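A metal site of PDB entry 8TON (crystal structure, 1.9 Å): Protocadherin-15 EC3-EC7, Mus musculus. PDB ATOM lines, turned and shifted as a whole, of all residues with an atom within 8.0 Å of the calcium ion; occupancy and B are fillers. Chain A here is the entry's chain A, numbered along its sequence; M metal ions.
OD1 of Asp 218 sits at hydrogen-bond distance from N of Arg 224 (2.9 Å).
O of Glu 135 sits at hydrogen-bond distance from ND2 of Asn 174.
NE of Arg 224 sits at hydrogen-bond distance from O of Asn 136.
OD2 of Asp 170 lies close to N of Asn 137.
The side-chain amide nitrogen (ND2) of Asn 136 lies within hydrogen-bond range of the backbone carbonyl oxygen (O) of His 222, 3.0 Å away.
The side-chain amide nitrogen (NE2) of Gln 138 sits at hydrogen-bond distance from the side-chain amide oxygen (OD1) of Asn 137 (3.2 Å).
Six residues have an atom within 4 Å of the calcium ion: Asn 136, Gln 138, Asp 168, Asp 170, Asn 174 and Asp 218.
Along chain A the residues within 4 Å of the calcium ion span positions 136 to 218.
The nearest printed residue that does not touch the calcium ion is Ala 139 (4.4 Å).
The calcium ion is bound by the backbone carbonyl oxygen (O) of Gln 138, the backbone carbonyl oxygen (O) of Asn 174, the side-chain carboxylate (OD2) of Asp 168, the side-chain amide oxygen (OD1) of Asn 136, the side-chain carboxylate (OD2) of Asp 218, the side-chain carboxylate (OD2) of Asp 170 and the side-chain carboxylate (OD1) of Asp 168.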
ATOM      1  N   GLU A 135       6.941  23.723  29.100  1.00  0.00           N
ATOM      2  CA  GLU A 135       7.867  23.392  28.044  1.00  0.00           C
ATOM      3  C   GLU A 135       8.997  22.492  28.591  1.00  0.00           C
ATOM      4  O   GLU A 135       9.479  22.641  29.696  1.00  0.00           O
ATOM      5  CB  GLU A 135       8.492  24.649  27.448  1.00  0.00           C
ATOM      6  CG  GLU A 135       9.532  24.269  26.420  1.00  0.00           C
ATOM      7  CD  GLU A 135       9.967  25.527  25.735  1.00  0.00           C
ATOM      8  OE1 GLU A 135      10.698  26.291  26.416  1.00  0.00           O
ATOM      9  OE2 GLU A 135       9.481  25.772  24.586  1.00  0.00           O
ATOM     10  N   ASN A 136       9.350  21.516  27.783  1.00  0.00           N
ATOM     11  CA  ASN A 136      10.387  20.555  28.086  1.00  0.00           C
ATOM     12  C   ASN A 136      11.640  21.122  27.426  1.00  0.00           C
ATOM     13  O   ASN A 136      11.884  20.980  26.207  1.00  0.00           O
ATOM     14  CB  ASN A 136      10.055  19.161  27.551  1.00  0.00           C
ATOM     15  CG  ASN A 136      11.193  18.220  27.879  1.00  0.00           C
ATOM     16  OD1 ASN A 136      11.902  18.416  28.877  1.00  0.00           O
ATOM     17  ND2 ASN A 136      11.340  17.176  27.079  1.00  0.00           N
ATOM     18  N   ASN A 137      12.322  21.914  28.234  1.00  0.00           N
ATOM     19  CA  ASN A 137      13.337  22.788  27.684  1.00  0.00           C
ATOM     20  C   ASN A 137      14.648  22.011  27.428  1.00  0.00           C
ATOM     21  O   ASN A 137      15.333  22.260  26.433  1.00  0.00           O
ATOM     22  CB  ASN A 137      13.495  23.978  28.625  1.00  0.00           C
ATOM     23  CG  ASN A 137      14.126  25.116  27.875  1.00  0.00           C
ATOM     24  OD1 ASN A 137      15.319  25.347  28.022  1.00  0.00           O
ATOM     25  ND2 ASN A 137      13.380  25.712  26.954  1.00  0.00           N
ATOM     26  N   GLN A 138      14.966  21.025  28.263  1.00  0.00           N
ATOM     27  CA  GLN A 138      16.295  20.365  28.208  1.00  0.00           C
ATOM     28  C   GLN A 138      16.176  18.841  28.127  1.00  0.00           C
ATOM     29  O   GLN A 138      15.270  18.265  28.732  1.00  0.00           O
ATOM     30  CB  GLN A 138      17.110  20.696  29.465  1.00  0.00           C
ATOM     31  CG  GLN A 138      17.477  22.168  29.603  1.00  0.00           C
ATOM     32  CD  GLN A 138      18.328  22.581  28.425  1.00  0.00           C
ATOM     33  OE1 GLN A 138      19.133  21.808  27.918  1.00  0.00           O
ATOM     34  NE2 GLN A 138      18.098  23.786  27.944  1.00  0.00           N
ATOM     35  N   ALA A 139      17.143  18.220  27.429  1.00  0.00           N
ATOM     36  CA  ALA A 139      17.375  16.794  27.370  1.00  0.00           C
ATOM     37  C   ALA A 139      18.147  16.300  28.587  1.00  0.00           C
ATOM     38  O   ALA A 139      18.888  17.044  29.227  1.00  0.00           O
ATOM     39  CB  ALA A 139      18.095  16.444  26.115  1.00  0.00           C
ATOM     40  N   PRO A 140      17.968  15.036  29.007  1.00  0.00           N
ATOM     41  CA  PRO A 140      18.784  14.524  30.110  1.00  0.00           C
ATOM     42  C   PRO A 140      20.276  14.643  29.772  1.00  0.00           C
ATOM     43  O   PRO A 140      20.647  14.620  28.616  1.00  0.00           O
ATOM     44  CB  PRO A 140      18.322  13.077  30.207  1.00  0.00           C
ATOM     45  CG  PRO A 140      16.865  13.166  29.729  1.00  0.00           C
ATOM     46  CD  PRO A 140      16.974  14.070  28.523  1.00  0.00           C
ATOM     47  N   VAL A 141      21.112  14.713  30.816  1.00  0.00           N
ATOM     48  CA  VAL A 141      22.536  14.889  30.651  1.00  0.00           C
ATOM     49  C   VAL A 141      23.241  13.823  31.489  1.00  0.00           C
ATOM     50  O   VAL A 141      22.989  13.716  32.661  1.00  0.00           O
ATOM     51  CB  VAL A 141      23.024  16.323  30.983  1.00  0.00           C
ATOM     52  CG1 VAL A 141      24.545  16.417  31.037  1.00  0.00           C
ATOM     53  CG2 VAL A 141      22.484  17.329  29.966  1.00  0.00           C
ATOM     54  N   THR A 167      20.853  13.192  34.549  1.00  0.00           N
ATOM     55  CA  THR A 167      19.937  14.095  35.221  1.00  0.00           C
ATOM     56  C   THR A 167      19.374  15.057  34.216  1.00  0.00           C
ATOM     57  O   THR A 167      19.925  15.245  33.129  1.00  0.00           O
ATOM     58  CB  THR A 167      20.638  14.867  36.342  1.00  0.00           C
ATOM     59  OG1 THR A 167      21.617  15.668  35.694  1.00  0.00           O
ATOM     60  CG2 THR A 167      21.307  13.965  37.335  1.00  0.00           C
ATOM     61  N   ASP A 168      18.262  15.684  34.595  1.00  0.00           N
ATOM     62  CA  ASP A 168      17.528  16.590  33.720  1.00  0.00           C
ATOM     63  C   ASP A 168      17.096  17.776  34.568  1.00  0.00           C
ATOM     64  O   ASP A 168      16.534  17.564  35.618  1.00  0.00           O
ATOM     65  CB  ASP A 168      16.271  15.926  33.141  1.00  0.00           C
ATOM     66  CG  ASP A 168      15.574  16.715  32.052  1.00  0.00           C
ATOM     67  OD1 ASP A 168      15.328  17.922  32.236  1.00  0.00           O
ATOM     68  OD2 ASP A 168      15.290  16.088  31.021  1.00  0.00           O
ATOM     69  N   PRO A 169      17.434  19.010  34.154  1.00  0.00           N
ATOM     70  CA  PRO A 169      17.150  20.210  34.934  1.00  0.00           C
ATOM     71  C   PRO A 169      15.660  20.557  35.011  1.00  0.00           C
ATOM     72  O   PRO A 169      15.222  21.139  36.001  1.00  0.00           O
ATOM     73  CB  PRO A 169      17.968  21.303  34.209  1.00  0.00           C
ATOM     74  CG  PRO A 169      18.117  20.807  32.789  1.00  0.00           C
ATOM     75  CD  PRO A 169      18.152  19.302  32.906  1.00  0.00           C
ATOM     76  N   ASP A 170      14.851  20.159  34.022  1.00  0.00           N
ATOM     77  CA  ASP A 170      13.472  20.611  33.966  1.00  0.00           C
ATOM     78  C   ASP A 170      12.681  20.160  35.183  1.00  0.00           C
ATOM     79  O   ASP A 170      13.015  19.211  35.877  1.00  0.00           O
ATOM     80  CB  ASP A 170      12.825  20.225  32.638  1.00  0.00           C
ATOM     81  CG  ASP A 170      13.554  20.787  31.444  1.00  0.00           C
ATOM     82  OD1 ASP A 170      14.130  21.851  31.597  1.00  0.00           O
ATOM     83  OD2 ASP A 170      13.564  20.151  30.369  1.00  0.00           O
ATOM     84  N   ALA A 171      11.578  20.874  35.440  1.00  0.00           N
ATOM     85  CA  ALA A 171      10.678  20.560  36.535  1.00  0.00           C
ATOM     86  C   ALA A 171       9.639  19.501  36.174  1.00  0.00           C
ATOM     87  O   ALA A 171       9.231  19.383  35.025  1.00  0.00           O
ATOM     88  CB  ALA A 171       9.996  21.861  36.959  1.00  0.00           C
ATOM     89  N   GLY A 172       9.201  18.750  37.200  1.00  0.00           N
ATOM     90  CA  GLY A 172       8.179  17.729  37.128  1.00  0.00           C
ATOM     91  C   GLY A 172       8.614  16.561  36.236  1.00  0.00           C
ATOM     92  O   GLY A 172       9.802  16.229  36.157  1.00  0.00           O
ATOM     93  N   ILE A 173       7.622  16.011  35.514  1.00  0.00           N
ATOM     94  CA  ILE A 173       7.809  14.906  34.586  1.00  0.00           C
ATOM     95  C   ILE A 173       8.873  15.243  33.533  1.00  0.00           C
ATOM     96  O   ILE A 173       9.542  14.315  33.063  1.00  0.00           O
ATOM     97  CB  ILE A 173       6.471  14.458  33.939  1.00  0.00           C
ATOM     98  CG1 ILE A 173       5.782  15.581  33.153  1.00  0.00           C
ATOM     99  CG2 ILE A 173       5.545  13.883  35.014  1.00  0.00           C
ATOM    100  CD1 ILE A 173       4.607  15.121  32.282  1.00  0.00           C
ATOM    101  N   ASN A 174       9.008  16.533  33.176  1.00  0.00           N
ATOM    102  CA  ASN A 174       9.967  17.007  32.195  1.00  0.00           C
ATOM    103  C   ASN A 174      11.420  16.814  32.646  1.00  0.00           C
ATOM    104  O   ASN A 174      12.359  16.957  31.826  1.00  0.00           O
ATOM    105  CB  ASN A 174       9.703  18.476  31.825  1.00  0.00           C
ATOM    106  CG  ASN A 174       8.425  18.685  31.051  1.00  0.00           C
ATOM    107  OD1 ASN A 174       7.651  17.768  30.725  1.00  0.00           O
ATOM    108  ND2 ASN A 174       8.194  19.937  30.698  1.00  0.00           N
ATOM    109  N   GLY A 175      11.611  16.532  33.946  1.00  0.00           N
ATOM    110  CA  GLY A 175      12.944  16.333  34.506  1.00  0.00           C
ATOM    111  C   GLY A 175      13.157  14.923  35.025  1.00  0.00           C
ATOM    112  O   GLY A 175      14.220  14.632  35.569  1.00  0.00           O
ATOM    113  N   GLN A 176      12.147  14.044  34.894  1.00  0.00           N
ATOM    114  CA  GLN A 176      12.240  12.660  35.356  1.00  0.00           C
ATOM    115  C   GLN A 176      12.883  11.766  34.293  1.00  0.00           C
ATOM    116  O   GLN A 176      12.420  11.731  33.154  1.00  0.00           O
ATOM    117  CB  GLN A 176      10.834  12.180  35.688  1.00  0.00           C
ATOM    118  CG  GLN A 176      10.357  12.821  36.977  1.00  0.00           C
ATOM    119  CD  GLN A 176       8.886  12.609  37.207  1.00  0.00           C
ATOM    120  OE1 GLN A 176       8.267  11.701  36.684  1.00  0.00           O
ATOM    121  NE2 GLN A 176       8.317  13.493  38.010  1.00  0.00           N
ATOM    122  N   VAL A 177      13.943  11.037  34.660  1.00  0.00           N
ATOM    123  CA  VAL A 177      14.776  10.336  33.676  1.00  0.00           C
ATOM    124  C   VAL A 177      14.434   8.853  33.621  1.00  0.00           C
ATOM    125  O   VAL A 177      14.316   8.234  34.669  1.00  0.00           O
ATOM    126  CB  VAL A 177      16.252  10.529  34.014  1.00  0.00           C
ATOM    127  CG1 VAL A 177      17.132   9.785  33.017  1.00  0.00           C
ATOM    128  CG2 VAL A 177      16.561  12.005  34.056  1.00  0.00           C
ATOM    129  N   THR A 217      15.733   9.252  28.502  1.00  0.00           N
ATOM    130  CA  THR A 217      14.568   9.985  28.010  1.00  0.00           C
ATOM    131  C   THR A 217      13.876  10.652  29.198  1.00  0.00           C
ATOM    132  O   THR A 217      13.715  10.026  30.253  1.00  0.00           O
ATOM    133  CB  THR A 217      13.609   9.005  27.331  1.00  0.00           C
ATOM    134  OG1 THR A 217      14.409   8.328  26.340  1.00  0.00           O
ATOM    135  CG2 THR A 217      12.411   9.709  26.768  1.00  0.00           C
ATOM    136  N   ASP A 218      13.331  11.865  29.023  1.00  0.00           N
ATOM    137  CA  ASP A 218      12.610  12.492  30.128  1.00  0.00           C
ATOM    138  C   ASP A 218      11.130  12.068  30.045  1.00  0.00           C
ATOM    139  O   ASP A 218      10.709  11.408  29.091  1.00  0.00           O
ATOM    140  CB  ASP A 218      12.874  14.001  30.183  1.00  0.00           C
ATOM    141  CG  ASP A 218      12.545  14.728  28.921  1.00  0.00           C
ATOM    142  OD1 ASP A 218      11.721  14.198  28.176  1.00  0.00           O
ATOM    143  OD2 ASP A 218      13.171  15.779  28.660  1.00  0.00           O
ATOM    144  N   GLY A 219      10.325  12.438  31.034  1.00  0.00           N
ATOM    145  CA  GLY A 219       8.938  11.999  31.110  1.00  0.00           C
ATOM    146  C   GLY A 219       7.957  12.984  30.492  1.00  0.00           C
ATOM    147  O   GLY A 219       6.773  12.867  30.725  1.00  0.00           O
ATOM    148  N   ALA A 220       8.418  13.857  29.576  1.00  0.00           N
ATOM    149  CA  ALA A 220       7.593  14.928  29.055  1.00  0.00           C
ATOM    150  C   ALA A 220       6.604  14.393  28.031  1.00  0.00           C
ATOM    151  O   ALA A 220       6.820  13.352  27.430  1.00  0.00           O
ATOM    152  CB  ALA A 220       8.403  16.048  28.479  1.00  0.00           C
ATOM    153  N   HIS A 222       6.353  15.841  25.310  1.00  0.00           N
ATOM    154  CA  HIS A 222       7.194  15.865  24.125  1.00  0.00           C
ATOM    155  C   HIS A 222       8.614  15.584  24.565  1.00  0.00           C
ATOM    156  O   HIS A 222       9.303  16.510  24.999  1.00  0.00           O
ATOM    157  CB  HIS A 222       7.141  17.222  23.405  1.00  0.00           C
ATOM    158  CG  HIS A 222       5.798  17.471  22.843  1.00  0.00           C
ATOM    159  ND1 HIS A 222       5.368  16.890  21.671  1.00  0.00           N
ATOM    160  CD2 HIS A 222       4.796  18.195  23.325  1.00  0.00           C
ATOM    161  CE1 HIS A 222       4.125  17.267  21.460  1.00  0.00           C
ATOM    162  NE2 HIS A 222       3.762  18.066  22.443  1.00  0.00           N
ATOM    163  N   PRO A 223       9.003  14.314  24.601  1.00  0.00           N
ATOM    164  CA  PRO A 223      10.221  13.917  25.303  1.00  0.00           C
ATOM    165  C   PRO A 223      11.472  14.400  24.622  1.00  0.00           C
ATOM    166  O   PRO A 223      11.500  14.585  23.396  1.00  0.00           O
ATOM    167  CB  PRO A 223      10.176  12.389  25.271  1.00  0.00           C
ATOM    168  CG  PRO A 223       9.316  12.052  24.071  1.00  0.00           C
ATOM    169  CD  PRO A 223       8.256  13.158  24.090  1.00  0.00           C
ATOM    170  N   ARG A 224      12.529  14.600  25.414  1.00  0.00           N
ATOM    171  CA  ARG A 224      13.866  14.779  24.840  1.00  0.00           C
ATOM    172  C   ARG A 224      14.749  13.592  25.280  1.00  0.00           C
ATOM    173  O   ARG A 224      14.502  12.939  26.314  1.00  0.00           O
ATOM    174  CB  ARG A 224      14.433  16.131  25.280  1.00  0.00           C
ATOM    175  CG  ARG A 224      13.789  17.349  24.592  1.00  0.00           C
ATOM    176  CD  ARG A 224      14.325  18.625  25.229  1.00  0.00           C
ATOM    177  NE  ARG A 224      13.667  19.775  24.663  1.00  0.00           N
ATOM    178  CZ  ARG A 224      14.068  20.403  23.562  1.00  0.00           C
ATOM    179  NH1 ARG A 224      13.501  21.530  23.184  1.00  0.00           N
ATOM    180  NH2 ARG A 224      15.078  19.934  22.868  1.00  0.00           N
ATOM    181  N   HIS A 225      15.800  13.341  24.516  1.00  0.00           N
ATOM    182  CA  HIS A 225      16.589  12.134  24.705  1.00  0.00           C
ATOM    183  C   HIS A 225      18.058  12.475  24.601  1.00  0.00           C
ATOM    184  O   HIS A 225      18.443  13.352  23.837  1.00  0.00           O
ATOM    185  CB  HIS A 225      16.325  11.137  23.555  1.00  0.00           C
ATOM    186  CG  HIS A 225      14.890  10.874  23.275  1.00  0.00           C
ATOM    187  ND1 HIS A 225      14.046   9.964  23.898  1.00  0.00           N
ATOM    188  CD2 HIS A 225      14.119  11.547  22.370  1.00  0.00           C
ATOM    189  CE1 HIS A 225      12.834  10.054  23.347  1.00  0.00           C
ATOM    190  NE2 HIS A 225      12.852  11.028  22.439  1.00  0.00           N
HETATM  191 CA    CA M   1      13.722  17.582  30.164  1.00  0.00          CA
